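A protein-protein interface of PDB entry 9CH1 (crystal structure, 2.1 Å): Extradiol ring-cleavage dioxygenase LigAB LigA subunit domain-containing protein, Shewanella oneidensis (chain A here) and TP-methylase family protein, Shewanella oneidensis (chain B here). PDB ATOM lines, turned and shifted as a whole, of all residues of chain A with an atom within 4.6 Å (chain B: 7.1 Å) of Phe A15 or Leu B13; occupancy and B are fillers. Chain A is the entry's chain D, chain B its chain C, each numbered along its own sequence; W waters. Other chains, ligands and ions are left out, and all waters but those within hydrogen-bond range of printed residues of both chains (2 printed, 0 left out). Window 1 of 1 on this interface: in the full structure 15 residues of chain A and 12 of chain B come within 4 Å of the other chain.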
ATOM      1  N   LEU A  11     -29.956   1.543  -7.251  1.00  0.00           N
ATOM      2  CA  LEU A  11     -30.320   1.435  -8.690  1.00  0.00           C
ATOM      3  C   LEU A  11     -29.138   0.846  -9.456  1.00  0.00           C
ATOM      4  O   LEU A  11     -29.291  -0.135 -10.177  1.00  0.00           O
ATOM      5  CB  LEU A  11     -30.713   2.809  -9.232  1.00  0.00           C
ATOM      6  CG  LEU A  11     -31.640   2.813 -10.453  1.00  0.00           C
ATOM      7  CD1 LEU A  11     -31.807   4.223 -10.996  1.00  0.00           C
ATOM      8  CD2 LEU A  11     -31.144   1.883 -11.544  1.00  0.00           C
ATOM      9  N   SER A  12     -27.959   1.450  -9.277  1.00  0.00           N
ATOM     10  CA  SER A  12     -26.747   0.999  -9.942  1.00  0.00           C
ATOM     11  C   SER A  12     -26.352  -0.384  -9.428  1.00  0.00           C
ATOM     12  O   SER A  12     -25.909  -1.232 -10.197  1.00  0.00           O
ATOM     13  CB  SER A  12     -25.625   1.994  -9.762  1.00  0.00           C
ATOM     14  OG  SER A  12     -24.409   1.506 -10.313  1.00  0.00           O
ATOM     15  N   ASP A  13     -26.523  -0.597  -8.118  1.00  0.00           N
ATOM     16  CA  ASP A  13     -26.195  -1.866  -7.491  1.00  0.00           C
ATOM     17  C   ASP A  13     -27.092  -2.961  -8.062  1.00  0.00           C
ATOM     18  O   ASP A  13     -26.625  -4.056  -8.368  1.00  0.00           O
ATOM     19  CB  ASP A  13     -26.298  -1.773  -5.976  1.00  0.00           C
ATOM     20  CG  ASP A  13     -25.188  -0.988  -5.292  1.00  0.00           C
ATOM     21  OD1 ASP A  13     -24.250  -0.563  -5.997  1.00  0.00           O
ATOM     22  OD2 ASP A  13     -25.269  -0.809  -4.059  1.00  0.00           O
ATOM     23  N   PHE A  14     -28.385  -2.647  -8.198  1.00  0.00           N
ATOM     24  CA  PHE A  14     -29.357  -3.585  -8.732  1.00  0.00           C
ATOM     25  C   PHE A  14     -28.941  -4.013 -10.136  1.00  0.00           C
ATOM     26  O   PHE A  14     -28.866  -5.204 -10.431  1.00  0.00           O
ATOM     27  CB  PHE A  14     -30.749  -2.944  -8.740  1.00  0.00           C
ATOM     28  CG  PHE A  14     -31.820  -3.794  -9.409  1.00  0.00           C
ATOM     29  CD1 PHE A  14     -32.056  -5.102  -9.000  1.00  0.00           C
ATOM     30  CD2 PHE A  14     -32.565  -3.292 -10.470  1.00  0.00           C
ATOM     31  CE1 PHE A  14     -33.025  -5.873  -9.620  1.00  0.00           C
ATOM     32  CE2 PHE A  14     -33.533  -4.068 -11.086  1.00  0.00           C
ATOM     33  CZ  PHE A  14     -33.759  -5.357 -10.663  1.00  0.00           C
ATOM     34  N   PHE A  15     -28.671  -3.028 -10.999  1.00  0.00           N
ATOM     35  CA  PHE A  15     -28.412  -3.289 -12.406  1.00  0.00           C
ATOM     36  C   PHE A  15     -27.166  -4.161 -12.554  1.00  0.00           C
ATOM     37  O   PHE A  15     -27.137  -5.055 -13.397  1.00  0.00           O
ATOM     38  CB  PHE A  15     -28.271  -1.987 -13.203  1.00  0.00           C
ATOM     39  CG  PHE A  15     -29.563  -1.210 -13.432  1.00  0.00           C
ATOM     40  CD1 PHE A  15     -30.805  -1.788 -13.190  1.00  0.00           C
ATOM     41  CD2 PHE A  15     -29.529   0.091 -13.921  1.00  0.00           C
ATOM     42  CE1 PHE A  15     -31.974  -1.075 -13.410  1.00  0.00           C
ATOM     43  CE2 PHE A  15     -30.701   0.799 -14.141  1.00  0.00           C
ATOM     44  CZ  PHE A  15     -31.920   0.215 -13.887  1.00  0.00           C
ATOM     45  N   THR A  16     -26.138  -3.896 -11.741  1.00  0.00           N
ATOM     46  CA  THR A  16     -24.898  -4.656 -11.815  1.00  0.00           C
ATOM     47  C   THR A  16     -25.176  -6.122 -11.487  1.00  0.00           C
ATOM     48  O   THR A  16     -24.665  -7.019 -12.155  1.00  0.00           O
ATOM     49  CB  THR A  16     -23.847  -4.060 -10.879  1.00  0.00           C
ATOM     50  OG1 THR A  16     -23.519  -2.786 -11.425  1.00  0.00           O
ATOM     51  CG2 THR A  16     -22.593  -4.911 -10.796  1.00  0.00           C
ATOM     52  N   GLN A  17     -25.989  -6.355 -10.450  1.00  0.00           N
ATOM     53  CA  GLN A  17     -26.334  -7.707 -10.036  1.00  0.00           C
ATOM     54  C   GLN A  17     -27.132  -8.387 -11.145  1.00  0.00           C
ATOM     55  O   GLN A  17     -26.853  -9.525 -11.512  1.00  0.00           O
ATOM     56  CB  GLN A  17     -27.176  -7.720  -8.760  1.00  0.00           C
ATOM     57  CG  GLN A  17     -26.506  -7.086  -7.546  1.00  0.00           C
ATOM     58  CD  GLN A  17     -27.377  -7.130  -6.308  1.00  0.00           C
ATOM     59  OE1 GLN A  17     -27.703  -8.203  -5.787  1.00  0.00           O
ATOM     60  NE2 GLN A  17     -27.770  -5.960  -5.826  1.00  0.00           N
ATOM     61  N   LEU A  18     -28.132  -7.666 -11.663  1.00  0.00           N
ATOM     62  CA  LEU A  18     -29.091  -8.216 -12.608  1.00  0.00           C
ATOM     63  C   LEU A  18     -28.379  -8.679 -13.876  1.00  0.00           C
ATOM     64  O   LEU A  18     -28.747  -9.696 -14.460  1.00  0.00           O
ATOM     65  CB  LEU A  18     -30.146  -7.151 -12.904  1.00  0.00           C
ATOM     66  CG  LEU A  18     -31.234  -7.533 -13.913  1.00  0.00           C
ATOM     67  CD1 LEU A  18     -31.998  -8.772 -13.482  1.00  0.00           C
ATOM     68  CD2 LEU A  18     -32.188  -6.368 -14.117  1.00  0.00           C
ATOM     69  N   GLY A  19     -27.361  -7.924 -14.298  1.00  0.00           N
ATOM     70  CA  GLY A  19     -26.651  -8.215 -15.534  1.00  0.00           C
ATOM     71  C   GLY A  19     -25.747  -9.438 -15.394  1.00  0.00           C
ATOM     72  O   GLY A  19     -25.428 -10.092 -16.384  1.00  0.00           O
ATOM     73  N   VAL A  49     -38.127   2.566 -16.230  1.00  0.00           N
ATOM     74  CA  VAL A  49     -37.749   1.267 -16.765  1.00  0.00           C
ATOM     75  C   VAL A  49     -38.855   0.779 -17.696  1.00  0.00           C
ATOM     76  O   VAL A  49     -38.578   0.274 -18.782  1.00  0.00           O
ATOM     77  CB  VAL A  49     -37.465   0.217 -15.673  1.00  0.00           C
ATOM     78  CG1 VAL A  49     -37.453  -1.196 -16.244  1.00  0.00           C
ATOM     79  CG2 VAL A  49     -36.169   0.501 -14.923  1.00  0.00           C
ATOM     80  N   LEU A  57     -33.351   7.369 -16.328  1.00  0.00           N
ATOM     81  CA  LEU A  57     -32.723   6.450 -15.392  1.00  0.00           C
ATOM     82  C   LEU A  57     -31.388   7.024 -14.925  1.00  0.00           C
ATOM     83  O   LEU A  57     -31.039   6.920 -13.751  1.00  0.00           O
ATOM     84  CB  LEU A  57     -32.534   5.075 -16.032  1.00  0.00           C
ATOM     85  CG  LEU A  57     -33.761   4.159 -16.044  1.00  0.00           C
ATOM     86  CD1 LEU A  57     -33.381   2.775 -16.542  1.00  0.00           C
ATOM     87  CD2 LEU A  57     -34.398   4.079 -14.666  1.00  0.00           C
ATOM     88  N   THR B   9     -15.550  -5.150 -22.735  1.00  0.00           N
ATOM     89  CA  THR B   9     -16.491  -5.347 -21.645  1.00  0.00           C
ATOM     90  C   THR B   9     -17.858  -5.741 -22.198  1.00  0.00           C
ATOM     91  O   THR B   9     -18.822  -5.858 -21.446  1.00  0.00           O
ATOM     92  CB  THR B   9     -16.578  -4.070 -20.809  1.00  0.00           C
ATOM     93  OG1 THR B   9     -17.087  -3.074 -21.690  1.00  0.00           O
ATOM     94  CG2 THR B   9     -15.233  -3.643 -20.249  1.00  0.00           C
ATOM     95  N   GLY B  10     -17.937  -5.937 -23.518  1.00  0.00           N
ATOM     96  CA  GLY B  10     -19.207  -6.228 -24.162  1.00  0.00           C
ATOM     97  C   GLY B  10     -20.092  -4.987 -24.187  1.00  0.00           C
ATOM     98  O   GLY B  10     -19.630  -3.891 -23.881  1.00  0.00           O
ATOM     99  N   LEU B  11     -21.369  -5.174 -24.539  1.00  0.00           N
ATOM    100  CA  LEU B  11     -22.307  -4.069 -24.648  1.00  0.00           C
ATOM    101  C   LEU B  11     -23.155  -3.970 -23.380  1.00  0.00           C
ATOM    102  O   LEU B  11     -23.405  -2.872 -22.891  1.00  0.00           O
ATOM    103  CB  LEU B  11     -23.164  -4.247 -25.901  1.00  0.00           C
ATOM    104  CG  LEU B  11     -22.556  -3.723 -27.207  1.00  0.00           C
ATOM    105  CD1 LEU B  11     -22.564  -2.204 -27.227  1.00  0.00           C
ATOM    106  CD2 LEU B  11     -21.143  -4.236 -27.416  1.00  0.00           C
ATOM    107  N   GLN B  12     -23.582  -5.121 -22.851  1.00  0.00           N
ATOM    108  CA  GLN B  12     -24.415  -5.165 -21.658  1.00  0.00           C
ATOM    109  C   GLN B  12     -23.561  -4.976 -20.405  1.00  0.00           C
ATOM    110  O   GLN B  12     -22.388  -5.339 -20.376  1.00  0.00           O
ATOM    111  CB  GLN B  12     -25.191  -6.479 -21.567  1.00  0.00           C
ATOM    112  CG  GLN B  12     -26.519  -6.479 -22.316  1.00  0.00           C
ATOM    113  CD  GLN B  12     -27.590  -5.665 -21.623  1.00  0.00           C
ATOM    114  OE1 GLN B  12     -27.325  -4.938 -20.660  1.00  0.00           O
ATOM    115  NE2 GLN B  12     -28.817  -5.774 -22.112  1.00  0.00           N
ATOM    116  N   LEU B  13     -24.191  -4.417 -19.367  1.00  0.00           N
ATOM    117  CA  LEU B  13     -23.536  -4.107 -18.106  1.00  0.00           C
ATOM    118  C   LEU B  13     -23.104  -5.381 -17.380  1.00  0.00           C
ATOM    119  O   LEU B  13     -23.914  -6.274 -17.134  1.00  0.00           O
ATOM    120  CB  LEU B  13     -24.522  -3.290 -17.272  1.00  0.00           C
ATOM    121  CG  LEU B  13     -24.067  -2.902 -15.861  1.00  0.00           C
ATOM    122  CD1 LEU B  13     -22.853  -1.991 -15.890  1.00  0.00           C
ATOM    123  CD2 LEU B  13     -25.214  -2.243 -15.115  1.00  0.00           C
ATOM    124  N   ALA B  14     -21.804  -5.444 -17.069  1.00  0.00           N
ATOM    125  CA  ALA B  14     -21.257  -6.310 -16.034  1.00  0.00           C
ATOM    126  C   ALA B  14     -21.128  -7.758 -16.505  1.00  0.00           C
ATOM    127  O   ALA B  14     -20.138  -8.416 -16.198  1.00  0.00           O
ATOM    128  CB  ALA B  14     -22.099  -6.215 -14.779  1.00  0.00           C
ATOM    129  N   GLY B  15     -22.127  -8.253 -17.242  1.00  0.00           N
ATOM    130  CA  GLY B  15     -22.262  -9.685 -17.456  1.00  0.00           C
ATOM    131  C   GLY B  15     -21.734 -10.149 -18.812  1.00  0.00           C
ATOM    132  O   GLY B  15     -21.625 -11.352 -19.043  1.00  0.00           O
ATOM    133  N   GLN B  16     -21.403  -9.211 -19.705  1.00  0.00           N
ATOM    134  CA  GLN B  16     -21.082  -9.578 -21.077  1.00  0.00           C
ATOM    135  C   GLN B  16     -19.568  -9.595 -21.294  1.00  0.00           C
ATOM    136  O   GLN B  16     -19.102  -9.898 -22.391  1.00  0.00           O
ATOM    137  CB  GLN B  16     -21.793  -8.665 -22.077  1.00  0.00           C
ATOM    138  CG  GLN B  16     -21.970  -9.295 -23.454  1.00  0.00           C
ATOM    139  CD  GLN B  16     -23.059  -8.645 -24.280  1.00  0.00           C
ATOM    140  OE1 GLN B  16     -23.022  -7.445 -24.568  1.00  0.00           O
ATOM    141  NE2 GLN B  16     -24.045  -9.439 -24.674  1.00  0.00           N
ATOM    142  N   ILE B  17     -18.803  -9.287 -20.242  1.00  0.00           N
ATOM    143  CA  ILE B  17     -17.357  -9.438 -20.290  1.00  0.00           C
ATOM    144  C   ILE B  17     -17.022 -10.909 -20.052  1.00  0.00           C
ATOM    145  O   ILE B  17     -17.775 -11.619 -19.390  1.00  0.00           O
ATOM    146  CB  ILE B  17     -16.667  -8.515 -19.268  1.00  0.00           C
ATOM    147  CG1 ILE B  17     -15.145  -8.532 -19.427  1.00  0.00           C
ATOM    148  CG2 ILE B  17     -17.088  -8.865 -17.839  1.00  0.00           C
ATOM    149  CD1 ILE B  17     -14.419  -7.516 -18.562  1.00  0.00           C
ATOM    150  N   ASP B  37     -21.639   4.211 -20.358  1.00  0.00           N
ATOM    151  CA  ASP B  37     -22.428   5.008 -19.432  1.00  0.00           C
ATOM    152  C   ASP B  37     -21.824   4.969 -18.030  1.00  0.00           C
ATOM    153  O   ASP B  37     -20.820   4.302 -17.792  1.00  0.00           O
ATOM    154  CB  ASP B  37     -23.873   4.537 -19.409  1.00  0.00           C
ATOM    155  CG  ASP B  37     -24.064   3.051 -19.144  1.00  0.00           C
ATOM    156  OD1 ASP B  37     -23.587   2.579 -18.090  1.00  0.00           O
ATOM    157  OD2 ASP B  37     -24.682   2.377 -19.997  1.00  0.00           O
ATOM    158  N   GLY B  38     -22.473   5.690 -17.108  1.00  0.00           N
ATOM    159  CA  GLY B  38     -21.991   5.848 -15.746  1.00  0.00           C
ATOM    160  C   GLY B  38     -22.271   4.615 -14.888  1.00  0.00           C
ATOM    161  O   GLY B  38     -21.625   4.419 -13.860  1.00  0.00           O
ATOM    162  N   PHE B  39     -23.243   3.797 -15.306  1.00  0.00           N
ATOM    163  CA  PHE B  39     -23.540   2.553 -14.612  1.00  0.00           C
ATOM    164  C   PHE B  39     -22.383   1.581 -14.822  1.00  0.00           C
ATOM    165  O   PHE B  39     -21.959   0.896 -13.893  1.00  0.00           O
ATOM    166  CB  PHE B  39     -24.845   1.908 -15.087  1.00  0.00           C
ATOM    167  CG  PHE B  39     -26.103   2.637 -14.639  1.00  0.00           C
ATOM    168  CD1 PHE B  39     -26.471   2.659 -13.299  1.00  0.00           C
ATOM    169  CD2 PHE B  39     -26.924   3.278 -15.558  1.00  0.00           C
ATOM    170  CE1 PHE B  39     -27.615   3.321 -12.890  1.00  0.00           C
ATOM    171  CE2 PHE B  39     -28.072   3.935 -15.143  1.00  0.00           C
ATOM    172  CZ  PHE B  39     -28.413   3.955 -13.811  1.00  0.00           C
ATOM    173  N   SER B  40     -21.894   1.523 -16.063  1.00  0.00           N
ATOM    174  CA  SER B  40     -20.791   0.648 -16.411  1.00  0.00           C
ATOM    175  C   SER B  40     -19.506   1.166 -15.771  1.00  0.00           C
ATOM    176  O   SER B  40     -18.619   0.386 -15.433  1.00  0.00           O
ATOM    177  CB  SER B  40     -20.657   0.517 -17.910  1.00  0.00           C
ATOM    178  OG  SER B  40     -19.568  -0.325 -18.258  1.00  0.00           O
ATOM    179  N   GLN B  41     -19.428   2.491 -15.598  1.00  0.00           N
ATOM    180  CA  GLN B  41     -18.252   3.133 -15.034  1.00  0.00           C
ATOM    181  C   GLN B  41     -18.128   2.772 -13.557  1.00  0.00           C
ATOM    182  O   GLN B  41     -17.037   2.472 -13.075  1.00  0.00           O
ATOM    183  CB  GLN B  41     -18.347   4.651 -15.195  1.00  0.00           C
ATOM    184  CG  GLN B  41     -17.018   5.378 -15.024  1.00  0.00           C
ATOM    185  CD  GLN B  41     -16.000   4.983 -16.070  1.00  0.00           C
ATOM    186  OE1 GLN B  41     -16.317   4.865 -17.258  1.00  0.00           O
ATOM    187  NE2 GLN B  41     -14.769   4.755 -15.639  1.00  0.00           N
ATOM    188  N   ARG B  42     -19.259   2.819 -12.845  1.00  0.00           N
ATOM    189  CA  ARG B  42     -19.294   2.495 -11.429  1.00  0.00           C
ATOM    190  C   ARG B  42     -18.906   1.031 -11.234  1.00  0.00           C
ATOM    191  O   ARG B  42     -18.099   0.708 -10.367  1.00  0.00           O
ATOM    192  CB  ARG B  42     -20.683   2.770 -10.843  1.00  0.00           C
ATOM    193  CG  ARG B  42     -21.023   4.246 -10.689  1.00  0.00           C
ATOM    194  CD  ARG B  42     -22.396   4.430 -10.065  1.00  0.00           C
ATOM    195  NE  ARG B  42     -22.815   5.835  -9.992  1.00  0.00           N
ATOM    196  CZ  ARG B  42     -23.810   6.360 -10.698  1.00  0.00           C
ATOM    197  NH1 ARG B  42     -24.435   5.634 -11.608  1.00  0.00           N
ATOM    198  NH2 ARG B  42     -24.165   7.618 -10.502  1.00  0.00           N
ATOM    199  N   TRP B  43     -19.497   0.154 -12.053  1.00  0.00           N
ATOM    200  CA  TRP B  43     -19.182  -1.263 -12.010  1.00  0.00           C
ATOM    201  C   TRP B  43     -17.671  -1.466 -12.099  1.00  0.00           C
ATOM    202  O   TRP B  43     -17.100  -2.252 -11.345  1.00  0.00           O
ATOM    203  CB  TRP B  43     -19.905  -2.010 -13.139  1.00  0.00           C
ATOM    204  CG  TRP B  43     -19.301  -3.353 -13.442  1.00  0.00           C
ATOM    205  CD1 TRP B  43     -19.501  -4.517 -12.762  1.00  0.00           C
ATOM    206  CD2 TRP B  43     -18.384  -3.667 -14.512  1.00  0.00           C
ATOM    207  NE1 TRP B  43     -18.775  -5.531 -13.327  1.00  0.00           N
ATOM    208  CE2 TRP B  43     -18.082  -5.042 -14.402  1.00  0.00           C
ATOM    209  CE3 TRP B  43     -17.795  -2.929 -15.545  1.00  0.00           C
ATOM    210  CZ2 TRP B  43     -17.219  -5.685 -15.286  1.00  0.00           C
ATOM    211  CZ3 TRP B  43     -16.945  -3.568 -16.419  1.00  0.00           C
ATOM    212  CH2 TRP B  43     -16.661  -4.926 -16.289  1.00  0.00           C
ATOM    213  N   LEU B  44     -17.033  -0.746 -13.028  1.00  0.00           N
ATOM    214  CA  LEU B  44     -15.604  -0.881 -13.257  1.00  0.00           C
ATOM    215  C   LEU B  44     -14.835  -0.475 -12.002  1.00  0.00           C
ATOM    216  O   LEU B  44     -13.910  -1.172 -11.585  1.00  0.00           O
ATOM    217  CB  LEU B  44     -15.177  -0.036 -14.457  1.00  0.00           C
ATOM    218  CG  LEU B  44     -13.688  -0.102 -14.815  1.00  0.00           C
ATOM    219  CD1 LEU B  44     -13.315  -1.490 -15.309  1.00  0.00           C
ATOM    220  CD2 LEU B  44     -13.312   0.951 -15.843  1.00  0.00           C
ATOM    221  N   ALA B 209     -28.737  -3.173 -26.467  1.00  0.00           N
ATOM    222  CA  ALA B 209     -28.975  -2.593 -25.155  1.00  0.00           C
ATOM    223  C   ALA B 209     -27.681  -2.571 -24.347  1.00  0.00           C
ATOM    224  O   ALA B 209     -26.844  -3.459 -24.488  1.00  0.00           O
ATOM    225  CB  ALA B 209     -30.051  -3.376 -24.435  1.00  0.00           C
ATOM    226  N   ASN B 210     -27.540  -1.557 -23.485  1.00  0.00           N
ATOM    227  CA  ASN B 210     -26.381  -1.439 -22.616  1.00  0.00           C
ATOM    228  C   ASN B 210     -26.763  -1.789 -21.178  1.00  0.00           C
ATOM    229  O   ASN B 210     -25.889  -2.031 -20.347  1.00  0.00           O
ATOM    230  CB  ASN B 210     -25.761  -0.046 -22.682  1.00  0.00           C
ATOM    231  CG  ASN B 210     -25.178   0.256 -24.042  1.00  0.00           C
ATOM    232  OD1 ASN B 210     -24.240  -0.419 -24.478  1.00  0.00           O
ATOM    233  ND2 ASN B 210     -25.708   1.262 -24.721  1.00  0.00           N
ATOM    234  N   LEU B 211     -28.070  -1.816 -20.894  1.00  0.00           N
ATOM    235  CA  LEU B 211     -28.552  -2.094 -19.550  1.00  0.00           C
ATOM    236  C   LEU B 211     -29.444  -3.332 -19.567  1.00  0.00           C
ATOM    237  O   LEU B 211     -30.119  -3.607 -20.558  1.00  0.00           O
ATOM    238  CB  LEU B 211     -29.291  -0.876 -18.998  1.00  0.00           C
ATOM    239  CG  LEU B 211     -28.452   0.391 -18.809  1.00  0.00           C
ATOM    240  CD1 LEU B 211     -29.314   1.537 -18.312  1.00  0.00           C
ATOM    241  CD2 LEU B 211     -27.289   0.142 -17.861  1.00  0.00           C
ATOM    242  N   PRO B 212     -29.478  -4.107 -18.459  1.00  0.00           N
ATOM    243  CA  PRO B 212     -30.241  -5.355 -18.407  1.00  0.00           C
ATOM    244  C   PRO B 212     -31.757  -5.174 -18.424  1.00  0.00           C
ATOM    245  O   PRO B 212     -32.490  -6.134 -18.652  1.00  0.00           O
ATOM    246  CB  PRO B 212     -29.750  -5.996 -17.094  1.00  0.00           C
ATOM    247  CG  PRO B 212     -29.354  -4.820 -16.229  1.00  0.00           C
ATOM    248  CD  PRO B 212     -28.765  -3.817 -17.205  1.00  0.00           C
ATOM    249  N   ILE B 213     -32.217  -3.939 -18.186  1.00  0.00           N
ATOM    250  CA  ILE B 213     -33.640  -3.640 -18.143  1.00  0.00           C
ATOM    251  C   ILE B 213     -34.069  -2.990 -19.456  1.00  0.00           C
ATOM    252  O   ILE B 213     -35.205  -2.536 -19.582  1.00  0.00           O
ATOM    253  CB  ILE B 213     -33.982  -2.749 -16.932  1.00  0.00           C
ATOM    254  CG1 ILE B 213     -33.108  -1.490 -16.873  1.00  0.00           C
ATOM    255  CG2 ILE B 213     -33.894  -3.547 -15.631  1.00  0.00           C
ATOM    256  CD1 ILE B 213     -33.189  -0.607 -18.104  1.00  0.00           C
HETATM  257  O   HOH W   1     -36.415  -0.398 -20.158  1.00  0.00           O
HETATM  258  O   HOH W   2     -24.010  -0.213 -12.145  1.00  0.00           O
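The backbone NH (N) of Leu B13 is in hydrogen-bond range of the backbone carbonyl oxygen (O) of Asn B210, 3.1 Å away.
The side-chain carboxylate (OD1) of Asp B37 lies within hydrogen-bond range of the backbone NH (N) of Phe B39.
The backbone carbonyl oxygen of Ser A12 lies within hydrogen-bond range of the side-chain hydroxyl of Thr A16 (3.1 Å).
Phe B39 touches Ser A12 (CD1 to CB, 3.7 Å).
CB of Phe A15 touches CD2 of Leu B13, 3.6 Å away.
Phe A15 touches Phe B39.
Pro B212 touches Phe A15 (CG to O, 3.6 Å).
Thr A16 touches Leu B13.
CG2 of Ile B213 touches CD2 of Leu A18, 3.6 Å away.
Gly A19 touches Leu B13 (CA to O, 3.7 Å).
Gly A19 touches Gly B15.
CG1 of Val A49 touches CB of Ile B213, 3.9 Å away.
Leu A57 touches Phe B39.
Of the printed residues of chain B, Phe A15 touches Leu B13 (3.6 Å), Phe B39 (3.9 Å), Pro B212 (3.6 Å) and Ile B213 (3.6 Å).
Leu B13 touches three residues of chain A.
Of the printed residues of chain B, Leu A57 touches Phe B39 (3.96 Å) and Ile B213 (3.7 Å).
Of the printed residues of chain B, Ser A12 touches Phe B39 (3.7 Å) and Arg B42 (3.6 Å).
Printed residues of chain A within 4 Å of Trp B43: Thr A16 (3.7 Å).
Gln B41 touches none of the printed residues of chain A.
The nearest residue of chain B that does not touch Phe A15 is Leu B211 (4.5 Å).
The nearest printed residue of chain B that does not touch Leu A57 is Leu B211 (4.6 Å).
Hydrophobic or aromatic side chains of chain B within 4 Å of the printed part of chain A: Leu B13, Ala B14, Phe B39, Trp B43, Pro B212 and Ile B213.
Among the printed residues, no Asp or Glu carboxylate lies within 4 Å of a Lys or Arg side-chain nitrogen of the other chain.
Water W1 lies within hydrogen-bond range of the backbone carbonyl oxygen of Ile B213 (2.5 Å) and the backbone carbonyl oxygen of Val A49 (2.7 Å).
Water W2 lies within hydrogen-bond range of OG of Ser A12 (2.5 Å), OG1 of Thr A16 (2.7 Å) and O of Phe B39 (2.9 Å).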
